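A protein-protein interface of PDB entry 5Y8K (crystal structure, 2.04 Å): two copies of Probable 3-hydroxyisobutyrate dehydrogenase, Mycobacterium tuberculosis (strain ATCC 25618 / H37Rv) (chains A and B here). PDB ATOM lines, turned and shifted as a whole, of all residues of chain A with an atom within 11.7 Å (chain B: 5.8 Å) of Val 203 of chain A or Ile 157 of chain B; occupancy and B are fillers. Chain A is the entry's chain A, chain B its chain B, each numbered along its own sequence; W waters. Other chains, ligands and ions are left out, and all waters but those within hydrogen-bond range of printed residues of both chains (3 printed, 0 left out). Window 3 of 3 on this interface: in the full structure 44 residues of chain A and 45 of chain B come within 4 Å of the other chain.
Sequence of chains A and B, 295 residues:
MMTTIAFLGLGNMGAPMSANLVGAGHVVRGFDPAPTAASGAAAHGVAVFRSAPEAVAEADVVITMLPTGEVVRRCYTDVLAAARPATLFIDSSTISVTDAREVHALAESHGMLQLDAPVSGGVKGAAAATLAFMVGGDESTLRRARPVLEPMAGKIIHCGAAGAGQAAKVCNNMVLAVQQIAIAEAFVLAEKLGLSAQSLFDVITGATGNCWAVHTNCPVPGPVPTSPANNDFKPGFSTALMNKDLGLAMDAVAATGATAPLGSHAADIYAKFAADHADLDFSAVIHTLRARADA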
ATOM      1  N   ILE A 183     -13.421   5.260 -22.710  1.00  0.00           N
ATOM      2  CA  ILE A 183     -13.796   6.282 -21.728  1.00  0.00           C
ATOM      3  C   ILE A 183     -14.879   7.207 -22.296  1.00  0.00           C
ATOM      4  O   ILE A 183     -15.855   7.501 -21.602  1.00  0.00           O
ATOM      5  CB  ILE A 183     -12.542   7.070 -21.248  1.00  0.00           C
ATOM      6  CG1 ILE A 183     -11.655   6.160 -20.389  1.00  0.00           C
ATOM      7  CG2 ILE A 183     -12.886   8.369 -20.530  1.00  0.00           C
ATOM      8  CD1 ILE A 183     -12.288   5.609 -19.143  1.00  0.00           C
ATOM      9  N   ALA A 186     -18.212   5.458 -22.251  1.00  0.00           N
ATOM     10  CA  ALA A 186     -18.682   5.400 -20.871  1.00  0.00           C
ATOM     11  C   ALA A 186     -19.322   6.712 -20.444  1.00  0.00           C
ATOM     12  O   ALA A 186     -20.401   6.691 -19.852  1.00  0.00           O
ATOM     13  CB  ALA A 186     -17.554   5.038 -19.920  1.00  0.00           C
ATOM     14  N   PHE A 187     -18.679   7.844 -20.749  1.00  0.00           N
ATOM     15  CA  PHE A 187     -19.267   9.148 -20.414  1.00  0.00           C
ATOM     16  C   PHE A 187     -20.558   9.450 -21.156  1.00  0.00           C
ATOM     17  O   PHE A 187     -21.460  10.020 -20.562  1.00  0.00           O
ATOM     18  CB  PHE A 187     -18.269  10.305 -20.554  1.00  0.00           C
ATOM     19  CG  PHE A 187     -17.375  10.438 -19.367  1.00  0.00           C
ATOM     20  CD1 PHE A 187     -17.835  11.057 -18.211  1.00  0.00           C
ATOM     21  CD2 PHE A 187     -16.089   9.903 -19.379  1.00  0.00           C
ATOM     22  CE1 PHE A 187     -17.032  11.152 -17.094  1.00  0.00           C
ATOM     23  CE2 PHE A 187     -15.282   9.999 -18.269  1.00  0.00           C
ATOM     24  CZ  PHE A 187     -15.755  10.624 -17.120  1.00  0.00           C
ATOM     25  N   ALA A 190     -23.242   7.119 -19.644  1.00  0.00           N
ATOM     26  CA  ALA A 190     -23.584   7.628 -18.322  1.00  0.00           C
ATOM     27  C   ALA A 190     -24.591   8.785 -18.407  1.00  0.00           C
ATOM     28  O   ALA A 190     -25.628   8.749 -17.756  1.00  0.00           O
ATOM     29  CB  ALA A 190     -22.329   8.055 -17.578  1.00  0.00           C
ATOM     30  N   GLY A 194     -28.576   9.131 -17.040  1.00  0.00           N
ATOM     31  CA  GLY A 194     -28.836  10.094 -15.967  1.00  0.00           C
ATOM     32  C   GLY A 194     -27.771  10.099 -14.869  1.00  0.00           C
ATOM     33  O   GLY A 194     -27.974  10.722 -13.824  1.00  0.00           O
ATOM     34  N   LEU A 195     -26.642   9.424 -15.112  1.00  0.00           N
ATOM     35  CA  LEU A 195     -25.498   9.430 -14.204  1.00  0.00           C
ATOM     36  C   LEU A 195     -24.612  10.618 -14.567  1.00  0.00           C
ATOM     37  O   LEU A 195     -24.146  10.691 -15.696  1.00  0.00           O
ATOM     38  CB  LEU A 195     -24.698   8.133 -14.364  1.00  0.00           C
ATOM     39  CG  LEU A 195     -23.441   7.938 -13.520  1.00  0.00           C
ATOM     40  CD1 LEU A 195     -23.793   7.873 -12.044  1.00  0.00           C
ATOM     41  CD2 LEU A 195     -22.715   6.668 -13.954  1.00  0.00           C
ATOM     42  N   SER A 196     -24.362  11.521 -13.625  1.00  0.00           N
ATOM     43  CA  SER A 196     -23.551  12.711 -13.900  1.00  0.00           C
ATOM     44  C   SER A 196     -22.084  12.381 -14.259  1.00  0.00           C
ATOM     45  O   SER A 196     -21.549  11.327 -13.874  1.00  0.00           O
ATOM     46  CB  SER A 196     -23.592  13.692 -12.726  1.00  0.00           C
ATOM     47  OG  SER A 196     -22.820  13.228 -11.635  1.00  0.00           O
ATOM     48  N   ALA A 197     -21.458  13.287 -15.006  1.00  0.00           N
ATOM     49  CA  ALA A 197     -20.060  13.130 -15.400  1.00  0.00           C
ATOM     50  C   ALA A 197     -19.153  13.053 -14.187  1.00  0.00           C
ATOM     51  O   ALA A 197     -18.262  12.216 -14.138  1.00  0.00           O
ATOM     52  CB  ALA A 197     -19.611  14.284 -16.301  1.00  0.00           C
ATOM     53  N   GLN A 198     -19.374  13.932 -13.214  1.00  0.00           N
ATOM     54  CA  GLN A 198     -18.594  13.910 -11.976  1.00  0.00           C
ATOM     55  C   GLN A 198     -18.744  12.579 -11.232  1.00  0.00           C
ATOM     56  O   GLN A 198     -17.746  12.039 -10.737  1.00  0.00           O
ATOM     57  CB  GLN A 198     -18.949  15.089 -11.055  1.00  0.00           C
ATOM     58  CG  GLN A 198     -17.992  15.271  -9.874  1.00  0.00           C
ATOM     59  CD  GLN A 198     -16.570  15.583 -10.321  1.00  0.00           C
ATOM     60  OE1 GLN A 198     -16.345  16.527 -11.085  1.00  0.00           O
ATOM     61  NE2 GLN A 198     -15.610  14.781  -9.869  1.00  0.00           N
ATOM     62  N   SER A 199     -19.960  12.031 -11.185  1.00  0.00           N
ATOM     63  CA  SER A 199     -20.182  10.750 -10.497  1.00  0.00           C
ATOM     64  C   SER A 199     -19.479   9.611 -11.187  1.00  0.00           C
ATOM     65  O   SER A 199     -18.852   8.794 -10.523  1.00  0.00           O
ATOM     66  CB  SER A 199     -21.664  10.415 -10.383  1.00  0.00           C
ATOM     67  OG  SER A 199     -22.282  11.335  -9.509  1.00  0.00           O
ATOM     68  N   LEU A 200     -19.598   9.548 -12.511  1.00  0.00           N
ATOM     69  CA  LEU A 200     -18.886   8.524 -13.274  1.00  0.00           C
ATOM     70  C   LEU A 200     -17.385   8.662 -13.069  1.00  0.00           C
ATOM     71  O   LEU A 200     -16.702   7.656 -12.815  1.00  0.00           O
ATOM     72  CB  LEU A 200     -19.204   8.565 -14.771  1.00  0.00           C
ATOM     73  CG  LEU A 200     -18.455   7.476 -15.571  1.00  0.00           C
ATOM     74  CD1 LEU A 200     -18.931   6.091 -15.134  1.00  0.00           C
ATOM     75  CD2 LEU A 200     -18.590   7.658 -17.080  1.00  0.00           C
ATOM     76  N   PHE A 201     -16.888   9.897 -13.180  1.00  0.00           N
ATOM     77  CA  PHE A 201     -15.465  10.195 -12.951  1.00  0.00           C
ATOM     78  C   PHE A 201     -14.978   9.675 -11.597  1.00  0.00           C
ATOM     79  O   PHE A 201     -13.968   8.957 -11.518  1.00  0.00           O
ATOM     80  CB  PHE A 201     -15.186  11.697 -13.075  1.00  0.00           C
ATOM     81  CG  PHE A 201     -13.745  12.058 -12.837  1.00  0.00           C
ATOM     82  CD1 PHE A 201     -12.836  12.056 -13.881  1.00  0.00           C
ATOM     83  CD2 PHE A 201     -13.284  12.377 -11.555  1.00  0.00           C
ATOM     84  CE1 PHE A 201     -11.504  12.371 -13.661  1.00  0.00           C
ATOM     85  CE2 PHE A 201     -11.943  12.695 -11.331  1.00  0.00           C
ATOM     86  CZ  PHE A 201     -11.054  12.695 -12.391  1.00  0.00           C
ATOM     87  N   ASP A 202     -15.703  10.029 -10.537  1.00  0.00           N
ATOM     88  CA  ASP A 202     -15.350   9.596  -9.177  1.00  0.00           C
ATOM     89  C   ASP A 202     -15.316   8.083  -9.078  1.00  0.00           C
ATOM     90  O   ASP A 202     -14.414   7.539  -8.451  1.00  0.00           O
ATOM     91  CB  ASP A 202     -16.325  10.145  -8.129  1.00  0.00           C
ATOM     92  CG  ASP A 202     -16.280  11.660  -8.015  1.00  0.00           C
ATOM     93  OD1 ASP A 202     -15.303  12.297  -8.457  1.00  0.00           O
ATOM     94  OD2 ASP A 202     -17.250  12.228  -7.498  1.00  0.00           O
ATOM     95  N   VAL A 203     -16.282   7.398  -9.700  1.00  0.00           N
ATOM     96  CA  VAL A 203     -16.329   5.935  -9.626  1.00  0.00           C
ATOM     97  C   VAL A 203     -15.162   5.327 -10.421  1.00  0.00           C
ATOM     98  O   VAL A 203     -14.363   4.582  -9.846  1.00  0.00           O
ATOM     99  CB  VAL A 203     -17.692   5.357 -10.083  1.00  0.00           C
ATOM    100  CG1 VAL A 203     -17.634   3.838 -10.193  1.00  0.00           C
ATOM    101  CG2 VAL A 203     -18.787   5.735  -9.086  1.00  0.00           C
ATOM    102  N   ILE A 204     -15.047   5.665 -11.712  1.00  0.00           N
ATOM    103  CA  ILE A 204     -14.037   5.035 -12.573  1.00  0.00           C
ATOM    104  C   ILE A 204     -12.633   5.259 -12.020  1.00  0.00           C
ATOM    105  O   ILE A 204     -11.854   4.308 -11.924  1.00  0.00           O
ATOM    106  CB  ILE A 204     -14.102   5.489 -14.055  1.00  0.00           C
ATOM    107  CG1 ILE A 204     -15.395   5.003 -14.693  1.00  0.00           C
ATOM    108  CG2 ILE A 204     -12.950   4.878 -14.865  1.00  0.00           C
ATOM    109  CD1 ILE A 204     -15.539   5.363 -16.181  1.00  0.00           C
ATOM    110  N   THR A 205     -12.313   6.495 -11.628  1.00  0.00           N
ATOM    111  CA  THR A 205     -10.962   6.787 -11.142  1.00  0.00           C
ATOM    112  C   THR A 205     -10.611   6.088  -9.832  1.00  0.00           C
ATOM    113  O   THR A 205      -9.435   5.871  -9.558  1.00  0.00           O
ATOM    114  CB  THR A 205     -10.691   8.288 -10.986  1.00  0.00           C
ATOM    115  OG1 THR A 205     -11.622   8.854 -10.061  1.00  0.00           O
ATOM    116  CG2 THR A 205     -10.776   8.988 -12.347  1.00  0.00           C
ATOM    117  N   GLY A 206     -11.624   5.726  -9.038  1.00  0.00           N
ATOM    118  CA  GLY A 206     -11.437   4.882  -7.861  1.00  0.00           C
ATOM    119  C   GLY A 206     -11.653   3.392  -8.086  1.00  0.00           C
ATOM    120  O   GLY A 206     -11.645   2.628  -7.121  1.00  0.00           O
ATOM    121  N   ALA A 207     -11.833   2.974  -9.342  1.00  0.00           N
ATOM    122  CA  ALA A 207     -12.168   1.585  -9.675  1.00  0.00           C
ATOM    123  C   ALA A 207     -11.259   1.015 -10.771  1.00  0.00           C
ATOM    124  O   ALA A 207     -10.286   1.651 -11.170  1.00  0.00           O
ATOM    125  CB  ALA A 207     -13.632   1.499 -10.084  1.00  0.00           C
ATOM    126  N   THR A 208     -11.585  -0.188 -11.244  1.00  0.00           N
ATOM    127  CA  THR A 208     -10.710  -0.938 -12.145  1.00  0.00           C
ATOM    128  C   THR A 208     -10.546  -0.330 -13.540  1.00  0.00           C
ATOM    129  O   THR A 208      -9.568  -0.615 -14.225  1.00  0.00           O
ATOM    130  CB  THR A 208     -11.197  -2.389 -12.315  1.00  0.00           C
ATOM    131  OG1 THR A 208     -12.572  -2.386 -12.704  1.00  0.00           O
ATOM    132  CG2 THR A 208     -11.013  -3.185 -11.000  1.00  0.00           C
ATOM    133  N   GLY A 209     -11.502   0.495 -13.955  1.00  0.00           N
ATOM    134  CA  GLY A 209     -11.455   1.140 -15.256  1.00  0.00           C
ATOM    135  C   GLY A 209     -10.531   2.344 -15.373  1.00  0.00           C
ATOM    136  O   GLY A 209     -10.352   2.853 -16.494  1.00  0.00           O
ATOM    137  N   ASN A 210      -9.950   2.792 -14.247  1.00  0.00           N
ATOM    138  CA  ASN A 210      -9.121   4.009 -14.221  1.00  0.00           C
ATOM    139  C   ASN A 210      -7.951   3.919 -15.176  1.00  0.00           C
ATOM    140  O   ASN A 210      -7.286   2.891 -15.256  1.00  0.00           O
ATOM    141  CB  ASN A 210      -8.560   4.266 -12.820  1.00  0.00           C
ATOM    142  CG  ASN A 210      -7.935   5.640 -12.682  1.00  0.00           C
ATOM    143  OD1 ASN A 210      -8.299   6.587 -13.378  1.00  0.00           O
ATOM    144  ND2 ASN A 210      -7.009   5.762 -11.758  1.00  0.00           N
ATOM    145  N   CYS A 211      -7.690   5.012 -15.870  1.00  0.00           N
ATOM    146  CA  CYS A 211      -6.546   5.122 -16.758  1.00  0.00           C
ATOM    147  C   CYS A 211      -6.352   6.589 -17.060  1.00  0.00           C
ATOM    148  O   CYS A 211      -7.247   7.411 -16.801  1.00  0.00           O
ATOM    149  CB  CYS A 211      -6.763   4.339 -18.065  1.00  0.00           C
ATOM    150  SG  CYS A 211      -8.286   4.776 -18.973  1.00  0.00           S
ATOM    151  N   VAL A 214      -9.010   8.930 -18.713  1.00  0.00           N
ATOM    152  CA  VAL A 214     -10.006   9.575 -17.844  1.00  0.00           C
ATOM    153  C   VAL A 214      -9.356  10.476 -16.775  1.00  0.00           C
ATOM    154  O   VAL A 214      -9.776  11.623 -16.613  1.00  0.00           O
ATOM    155  CB  VAL A 214     -11.054   8.574 -17.240  1.00  0.00           C
ATOM    156  CG1 VAL A 214     -10.422   7.439 -16.449  1.00  0.00           C
ATOM    157  CG2 VAL A 214     -12.065   9.320 -16.377  1.00  0.00           C
ATOM    158  N   HIS A 215      -8.342   9.996 -16.052  1.00  0.00           N
ATOM    159  CA  HIS A 215      -7.878  10.761 -14.872  1.00  0.00           C
ATOM    160  C   HIS A 215      -7.136  12.044 -15.239  1.00  0.00           C
ATOM    161  O   HIS A 215      -7.120  12.990 -14.456  1.00  0.00           O
ATOM    162  CB  HIS A 215      -7.116   9.908 -13.826  1.00  0.00           C
ATOM    163  CG  HIS A 215      -5.781   9.372 -14.265  1.00  0.00           C
ATOM    164  ND1 HIS A 215      -4.704  10.177 -14.566  1.00  0.00           N
ATOM    165  CD2 HIS A 215      -5.323   8.096 -14.340  1.00  0.00           C
ATOM    166  CE1 HIS A 215      -3.656   9.420 -14.858  1.00  0.00           C
ATOM    167  NE2 HIS A 215      -4.008   8.155 -14.732  1.00  0.00           N
ATOM    168  N   CYS A 218      -9.761  13.460 -19.368  1.00  0.00           N
ATOM    169  CA  CYS A 218     -11.228  13.372 -19.289  1.00  0.00           C
ATOM    170  C   CYS A 218     -11.941  14.132 -20.419  1.00  0.00           C
ATOM    171  O   CYS A 218     -11.816  15.366 -20.501  1.00  0.00           O
ATOM    172  CB  CYS A 218     -11.698  13.936 -17.946  1.00  0.00           C
ATOM    173  SG  CYS A 218     -13.466  13.778 -17.699  1.00  0.00           S
ATOM    174  N   VAL A 220     -14.999  14.997 -21.060  1.00  0.00           N
ATOM    175  CA  VAL A 220     -16.095  15.909 -20.741  1.00  0.00           C
ATOM    176  C   VAL A 220     -15.552  17.016 -19.845  1.00  0.00           C
ATOM    177  O   VAL A 220     -14.695  16.746 -19.008  1.00  0.00           O
ATOM    178  CB  VAL A 220     -17.291  15.194 -20.072  1.00  0.00           C
ATOM    179  CG1 VAL A 220     -17.837  14.125 -21.008  1.00  0.00           C
ATOM    180  CG2 VAL A 220     -16.927  14.582 -18.729  1.00  0.00           C
ATOM    181  N   PRO A 223     -14.591  17.597 -14.594  1.00  0.00           N
ATOM    182  CA  PRO A 223     -13.854  16.774 -13.611  1.00  0.00           C
ATOM    183  C   PRO A 223     -12.339  16.944 -13.546  1.00  0.00           C
ATOM    184  O   PRO A 223     -11.739  16.693 -12.507  1.00  0.00           O
ATOM    185  CB  PRO A 223     -14.204  15.355 -14.022  1.00  0.00           C
ATOM    186  CG  PRO A 223     -15.563  15.490 -14.658  1.00  0.00           C
ATOM    187  CD  PRO A 223     -15.539  16.796 -15.387  1.00  0.00           C
ATOM    188  N   VAL A 224     -11.719  17.335 -14.649  1.00  0.00           N
ATOM    189  CA  VAL A 224     -10.276  17.571 -14.695  1.00  0.00           C
ATOM    190  C   VAL A 224     -10.132  18.907 -15.429  1.00  0.00           C
ATOM    191  O   VAL A 224     -10.116  18.930 -16.663  1.00  0.00           O
ATOM    192  CB  VAL A 224      -9.562  16.436 -15.450  1.00  0.00           C
ATOM    193  CG1 VAL A 224      -8.060  16.712 -15.572  1.00  0.00           C
ATOM    194  CG2 VAL A 224      -9.840  15.094 -14.777  1.00  0.00           C
ATOM    195  N   ALA B 132     -16.802  -2.687  -2.730  1.00  0.00           N
ATOM    196  CA  ALA B 132     -17.223  -1.309  -3.028  1.00  0.00           C
ATOM    197  C   ALA B 132     -18.705  -1.326  -3.343  1.00  0.00           C
ATOM    198  O   ALA B 132     -19.102  -2.019  -4.265  1.00  0.00           O
ATOM    199  CB  ALA B 132     -16.455  -0.743  -4.205  1.00  0.00           C
ATOM    200  N   PHE B 133     -19.509  -0.591  -2.577  1.00  0.00           N
ATOM    201  CA  PHE B 133     -20.925  -0.395  -2.877  1.00  0.00           C
ATOM    202  C   PHE B 133     -21.069   0.884  -3.690  1.00  0.00           C
ATOM    203  O   PHE B 133     -20.602   1.964  -3.281  1.00  0.00           O
ATOM    204  CB  PHE B 133     -21.786  -0.302  -1.602  1.00  0.00           C
ATOM    205  CG  PHE B 133     -21.906  -1.603  -0.832  1.00  0.00           C
ATOM    206  CD1 PHE B 133     -23.072  -2.365  -0.891  1.00  0.00           C
ATOM    207  CD2 PHE B 133     -20.862  -2.065  -0.044  1.00  0.00           C
ATOM    208  CE1 PHE B 133     -23.185  -3.566  -0.204  1.00  0.00           C
ATOM    209  CE2 PHE B 133     -20.979  -3.272   0.665  1.00  0.00           C
ATOM    210  CZ  PHE B 133     -22.137  -4.019   0.575  1.00  0.00           C
ATOM    211  N   MET B 134     -21.727   0.750  -4.839  1.00  0.00           N
ATOM    212  CA  MET B 134     -22.054   1.866  -5.695  1.00  0.00           C
ATOM    213  C   MET B 134     -23.553   2.086  -5.577  1.00  0.00           C
ATOM    214  O   MET B 134     -24.327   1.280  -6.052  1.00  0.00           O
ATOM    215  CB  MET B 134     -21.616   1.553  -7.123  1.00  0.00           C
ATOM    216  CG  MET B 134     -20.099   1.610  -7.282  1.00  0.00           C
ATOM    217  SD  MET B 134     -19.497   0.588  -8.621  1.00  0.00           S
ATOM    218  CE  MET B 134     -19.610  -1.051  -7.896  1.00  0.00           C
ATOM    219  N   VAL B 135     -23.936   3.182  -4.920  1.00  0.00           N
ATOM    220  CA  VAL B 135     -25.295   3.407  -4.424  1.00  0.00           C
ATOM    221  C   VAL B 135     -26.043   4.463  -5.239  1.00  0.00           C
ATOM    222  O   VAL B 135     -25.507   5.541  -5.534  1.00  0.00           O
ATOM    223  CB  VAL B 135     -25.285   3.853  -2.945  1.00  0.00           C
ATOM    224  CG1 VAL B 135     -26.705   4.128  -2.433  1.00  0.00           C
ATOM    225  CG2 VAL B 135     -24.602   2.799  -2.087  1.00  0.00           C
ATOM    226  N   GLY B 136     -27.282   4.139  -5.589  1.00  0.00           N
ATOM    227  CA  GLY B 136     -28.234   5.083  -6.171  1.00  0.00           C
ATOM    228  C   GLY B 136     -29.431   5.199  -5.251  1.00  0.00           C
ATOM    229  O   GLY B 136     -29.856   4.214  -4.646  1.00  0.00           O
ATOM    230  N   LEU B 142     -29.425   6.736   2.126  1.00  0.00           N
ATOM    231  CA  LEU B 142     -28.054   6.209   2.252  1.00  0.00           C
ATOM    232  C   LEU B 142     -27.505   6.415   3.668  1.00  0.00           C
ATOM    233  O   LEU B 142     -26.875   5.520   4.219  1.00  0.00           O
ATOM    234  CB  LEU B 142     -27.101   6.853   1.232  1.00  0.00           C
ATOM    235  CG  LEU B 142     -25.633   6.416   1.305  1.00  0.00           C
ATOM    236  CD1 LEU B 142     -25.487   4.906   1.272  1.00  0.00           C
ATOM    237  CD2 LEU B 142     -24.830   7.059   0.196  1.00  0.00           C
ATOM    238  N   LYS B 155     -15.484   0.379   0.506  1.00  0.00           N
ATOM    239  CA  LYS B 155     -15.907   1.687   0.027  1.00  0.00           C
ATOM    240  C   LYS B 155     -17.433   1.746  -0.169  1.00  0.00           C
ATOM    241  O   LYS B 155     -18.064   0.769  -0.603  1.00  0.00           O
ATOM    242  CB  LYS B 155     -15.225   1.980  -1.299  1.00  0.00           C
ATOM    243  CG  LYS B 155     -15.543   3.354  -1.841  1.00  0.00           C
ATOM    244  N   ILE B 156     -18.003   2.902   0.160  1.00  0.00           N
ATOM    245  CA  ILE B 156     -19.403   3.222  -0.119  1.00  0.00           C
ATOM    246  C   ILE B 156     -19.400   4.541  -0.877  1.00  0.00           C
ATOM    247  O   ILE B 156     -18.955   5.564  -0.350  1.00  0.00           O
ATOM    248  CB  ILE B 156     -20.230   3.381   1.176  1.00  0.00           C
ATOM    249  CG1 ILE B 156     -20.167   2.099   2.018  1.00  0.00           C
ATOM    250  CG2 ILE B 156     -21.674   3.757   0.839  1.00  0.00           C
ATOM    251  CD1 ILE B 156     -20.736   2.241   3.425  1.00  0.00           C
ATOM    252  N   ILE B 157     -19.888   4.512  -2.109  1.00  0.00           N
ATOM    253  CA  ILE B 157     -19.908   5.699  -2.933  1.00  0.00           C
ATOM    254  C   ILE B 157     -21.317   5.967  -3.461  1.00  0.00           C
ATOM    255  O   ILE B 157     -21.967   5.105  -4.051  1.00  0.00           O
ATOM    256  CB  ILE B 157     -18.808   5.669  -4.028  1.00  0.00           C
ATOM    257  CG1 ILE B 157     -18.964   6.850  -5.005  1.00  0.00           C
ATOM    258  CG2 ILE B 157     -18.763   4.332  -4.756  1.00  0.00           C
ATOM    259  CD1 ILE B 157     -17.675   7.228  -5.721  1.00  0.00           C
ATOM    260  N   HIS B 158     -21.777   7.184  -3.214  1.00  0.00           N
ATOM    261  CA  HIS B 158     -23.081   7.638  -3.660  1.00  0.00           C
ATOM    262  C   HIS B 158     -22.988   8.139  -5.101  1.00  0.00           C
ATOM    263  O   HIS B 158     -22.333   9.155  -5.370  1.00  0.00           O
ATOM    264  CB  HIS B 158     -23.570   8.760  -2.747  1.00  0.00           C
ATOM    265  CG  HIS B 158     -24.934   9.257  -3.088  1.00  0.00           C
ATOM    266  ND1 HIS B 158     -25.994   8.411  -3.313  1.00  0.00           N
ATOM    267  CD2 HIS B 158     -25.413  10.510  -3.249  1.00  0.00           C
ATOM    268  CE1 HIS B 158     -27.072   9.117  -3.587  1.00  0.00           C
ATOM    269  NE2 HIS B 158     -26.750  10.395  -3.547  1.00  0.00           N
ATOM    270  N   CYS B 159     -23.666   7.441  -6.010  1.00  0.00           N
ATOM    271  CA  CYS B 159     -23.570   7.708  -7.443  1.00  0.00           C
ATOM    272  C   CYS B 159     -24.642   8.619  -8.000  1.00  0.00           C
ATOM    273  O   CYS B 159     -24.467   9.132  -9.095  1.00  0.00           O
ATOM    274  CB  CYS B 159     -23.592   6.404  -8.215  1.00  0.00           C
ATOM    275  SG  CYS B 159     -22.209   5.367  -7.753  1.00  0.00           S
ATOM    276  N   ALA B 168     -23.218   3.255 -12.774  1.00  0.00           N
ATOM    277  CA  ALA B 168     -21.791   3.446 -12.549  1.00  0.00           C
ATOM    278  C   ALA B 168     -21.009   2.150 -12.675  1.00  0.00           C
ATOM    279  O   ALA B 168     -19.949   2.126 -13.298  1.00  0.00           O
ATOM    280  CB  ALA B 168     -21.536   4.063 -11.190  1.00  0.00           C
ATOM    281  N   LYS B 169     -21.529   1.087 -12.073  1.00  0.00           N
ATOM    282  CA  LYS B 169     -20.886  -0.201 -12.134  1.00  0.00           C
ATOM    283  C   LYS B 169     -20.791  -0.679 -13.583  1.00  0.00           C
ATOM    284  O   LYS B 169     -19.714  -1.070 -14.029  1.00  0.00           O
ATOM    285  CB  LYS B 169     -21.636  -1.246 -11.302  1.00  0.00           C
ATOM    286  CG  LYS B 169     -20.957  -2.598 -11.371  1.00  0.00           C
ATOM    287  CD  LYS B 169     -21.510  -3.619 -10.404  1.00  0.00           C
ATOM    288  CE  LYS B 169     -20.811  -4.940 -10.683  1.00  0.00           C
ATOM    289  NZ  LYS B 169     -21.206  -5.991  -9.718  1.00  0.00           N
ATOM    290  N   ASN B 172     -18.257   1.292 -15.677  1.00  0.00           N
ATOM    291  CA  ASN B 172     -16.875   0.931 -15.329  1.00  0.00           C
ATOM    292  C   ASN B 172     -16.514  -0.425 -15.908  1.00  0.00           C
ATOM    293  O   ASN B 172     -15.461  -0.575 -16.512  1.00  0.00           O
ATOM    294  CB  ASN B 172     -16.656   0.921 -13.818  1.00  0.00           C
ATOM    295  CG  ASN B 172     -15.264   0.487 -13.450  1.00  0.00           C
ATOM    296  OD1 ASN B 172     -14.326   1.276 -13.505  1.00  0.00           O
ATOM    297  ND2 ASN B 172     -15.112  -0.772 -13.094  1.00  0.00           N
HETATM  298  O   HOH W   1     -22.451  11.388  -6.977  1.00  0.00           O
HETATM  299  O   HOH W   2     -20.124   8.757  -7.543  1.00  0.00           O
HETATM  300  O   HOH W   3     -25.272  11.102 -10.943  1.00  0.00           O
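OG of Ser 199 of chain A lies within hydrogen-bond range of O of Cys 159 of chain B (3.1 Å). The side-chain hydroxyl of Thr 208 of chain A sits at hydrogen-bond distance from the side-chain amide nitrogen of Asn 172 of chain B. The side-chain amide oxygen (OD1) of Asn 172 of chain B sits at hydrogen-bond distance from the backbone NH (N) of Gly 209 of chain A (3.0 Å).
The side-chain hydroxyl (OG) of Ser 199 of chain A lies within hydrogen-bond range of the side-chain hydroxyl (OG) of Ser 196 of chain A (2.9 Å). The backbone carbonyl oxygen (O) of Val 135 of chain B is in hydrogen-bond range of the backbone NH (N) of Cys 159 of chain B (2.7 Å). The backbone carbonyl oxygen of Ile 157 of chain B lies within hydrogen-bond range of the side-chain sulfur of Cys 159 of chain B (3.7 Å).
Leu 195 of chain A touches Cys 159 of chain B (CD1 to O, 3.3 Å). Leu 195 of chain A touches Ala 168 of chain B (CD2 to CA, 3.6 Å). Val 203 of chain A touches Ile 157 of chain B (CG2 to CD1, 3.8 Å). Val 203 of chain A touches Cys 159 of chain B. CG2 of Val 203 of chain A touches CB of Ala 168 of chain B, at 3.8 Å. CB of Ala 207 of chain A touches OD1 of Asn 172 of chain B, 3.5 Å away.
Val 203 of chain A touches just these residues of chain B: Ile 157 (3.8 Å), Cys 159 (3.7 Å) and Ala 168 (3.8 Å). No residue of chain A comes within 4 Å of Val 135 of chain B. No residue of chain A comes within 4 Å of Lys 155 of chain B. Cys 159 of chain B touches just these residues of chain A: Leu 195, Ser 199 and Val 203. Ala 168 of chain B touches two residues of chain A. Of the printed residues of chain B, Ile 204 of chain A touches Asn 172 (3.9 Å). Printed residues of chain B within 4 Å of Leu 195 of chain A: Cys 159 (3.3 Å) and Ala 168 (3.6 Å). Printed residues of chain B within 4 Å of Ala 207 of chain A: Asn 172 (3.5 Å). Phe 187 of chain A touches none of the printed residues of chain B. The nearest residue of chain B that does not touch Val 203 of chain A is Met 134 of chain B (4.1 Å). The nearest printed residue of chain A that does not touch Ile 157 of chain B is Asp 202 of chain A (4.02 Å).
Hydrophobic or aromatic side chains of chain A that line the printed part of chain B: Leu 195, Val 203 and Ala 207. Along chain A the printed residues that touch a printed residue of chain B span positions 195 to 209. Among the printed residues, no Asp or Glu carboxylate lies within 4 Å of a Lys or Arg side-chain nitrogen of the other chain.
No position is printed for both chains. Of the 10 pairs that touch across the chains among the printed residues, none has its exchanged pair printed and touching as well.
Water W1 lies within hydrogen-bond range of the side-chain hydroxyl (OG) of Ser 199 of chain A (2.5 Å) and the backbone carbonyl oxygen (O) of His 158 of chain B (2.8 Å). Water W3 lies within hydrogen-bond range of O of Cys 159 of chain B (2.8 Å), N of Ser 196 of chain A (2.9 Å) and OG of Ser 199 of chain A (3.3 Å). Water W2 bridges O of His 158 of chain B (3.1 Å) and O of Ser 199 of chain A (3.2 Å).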
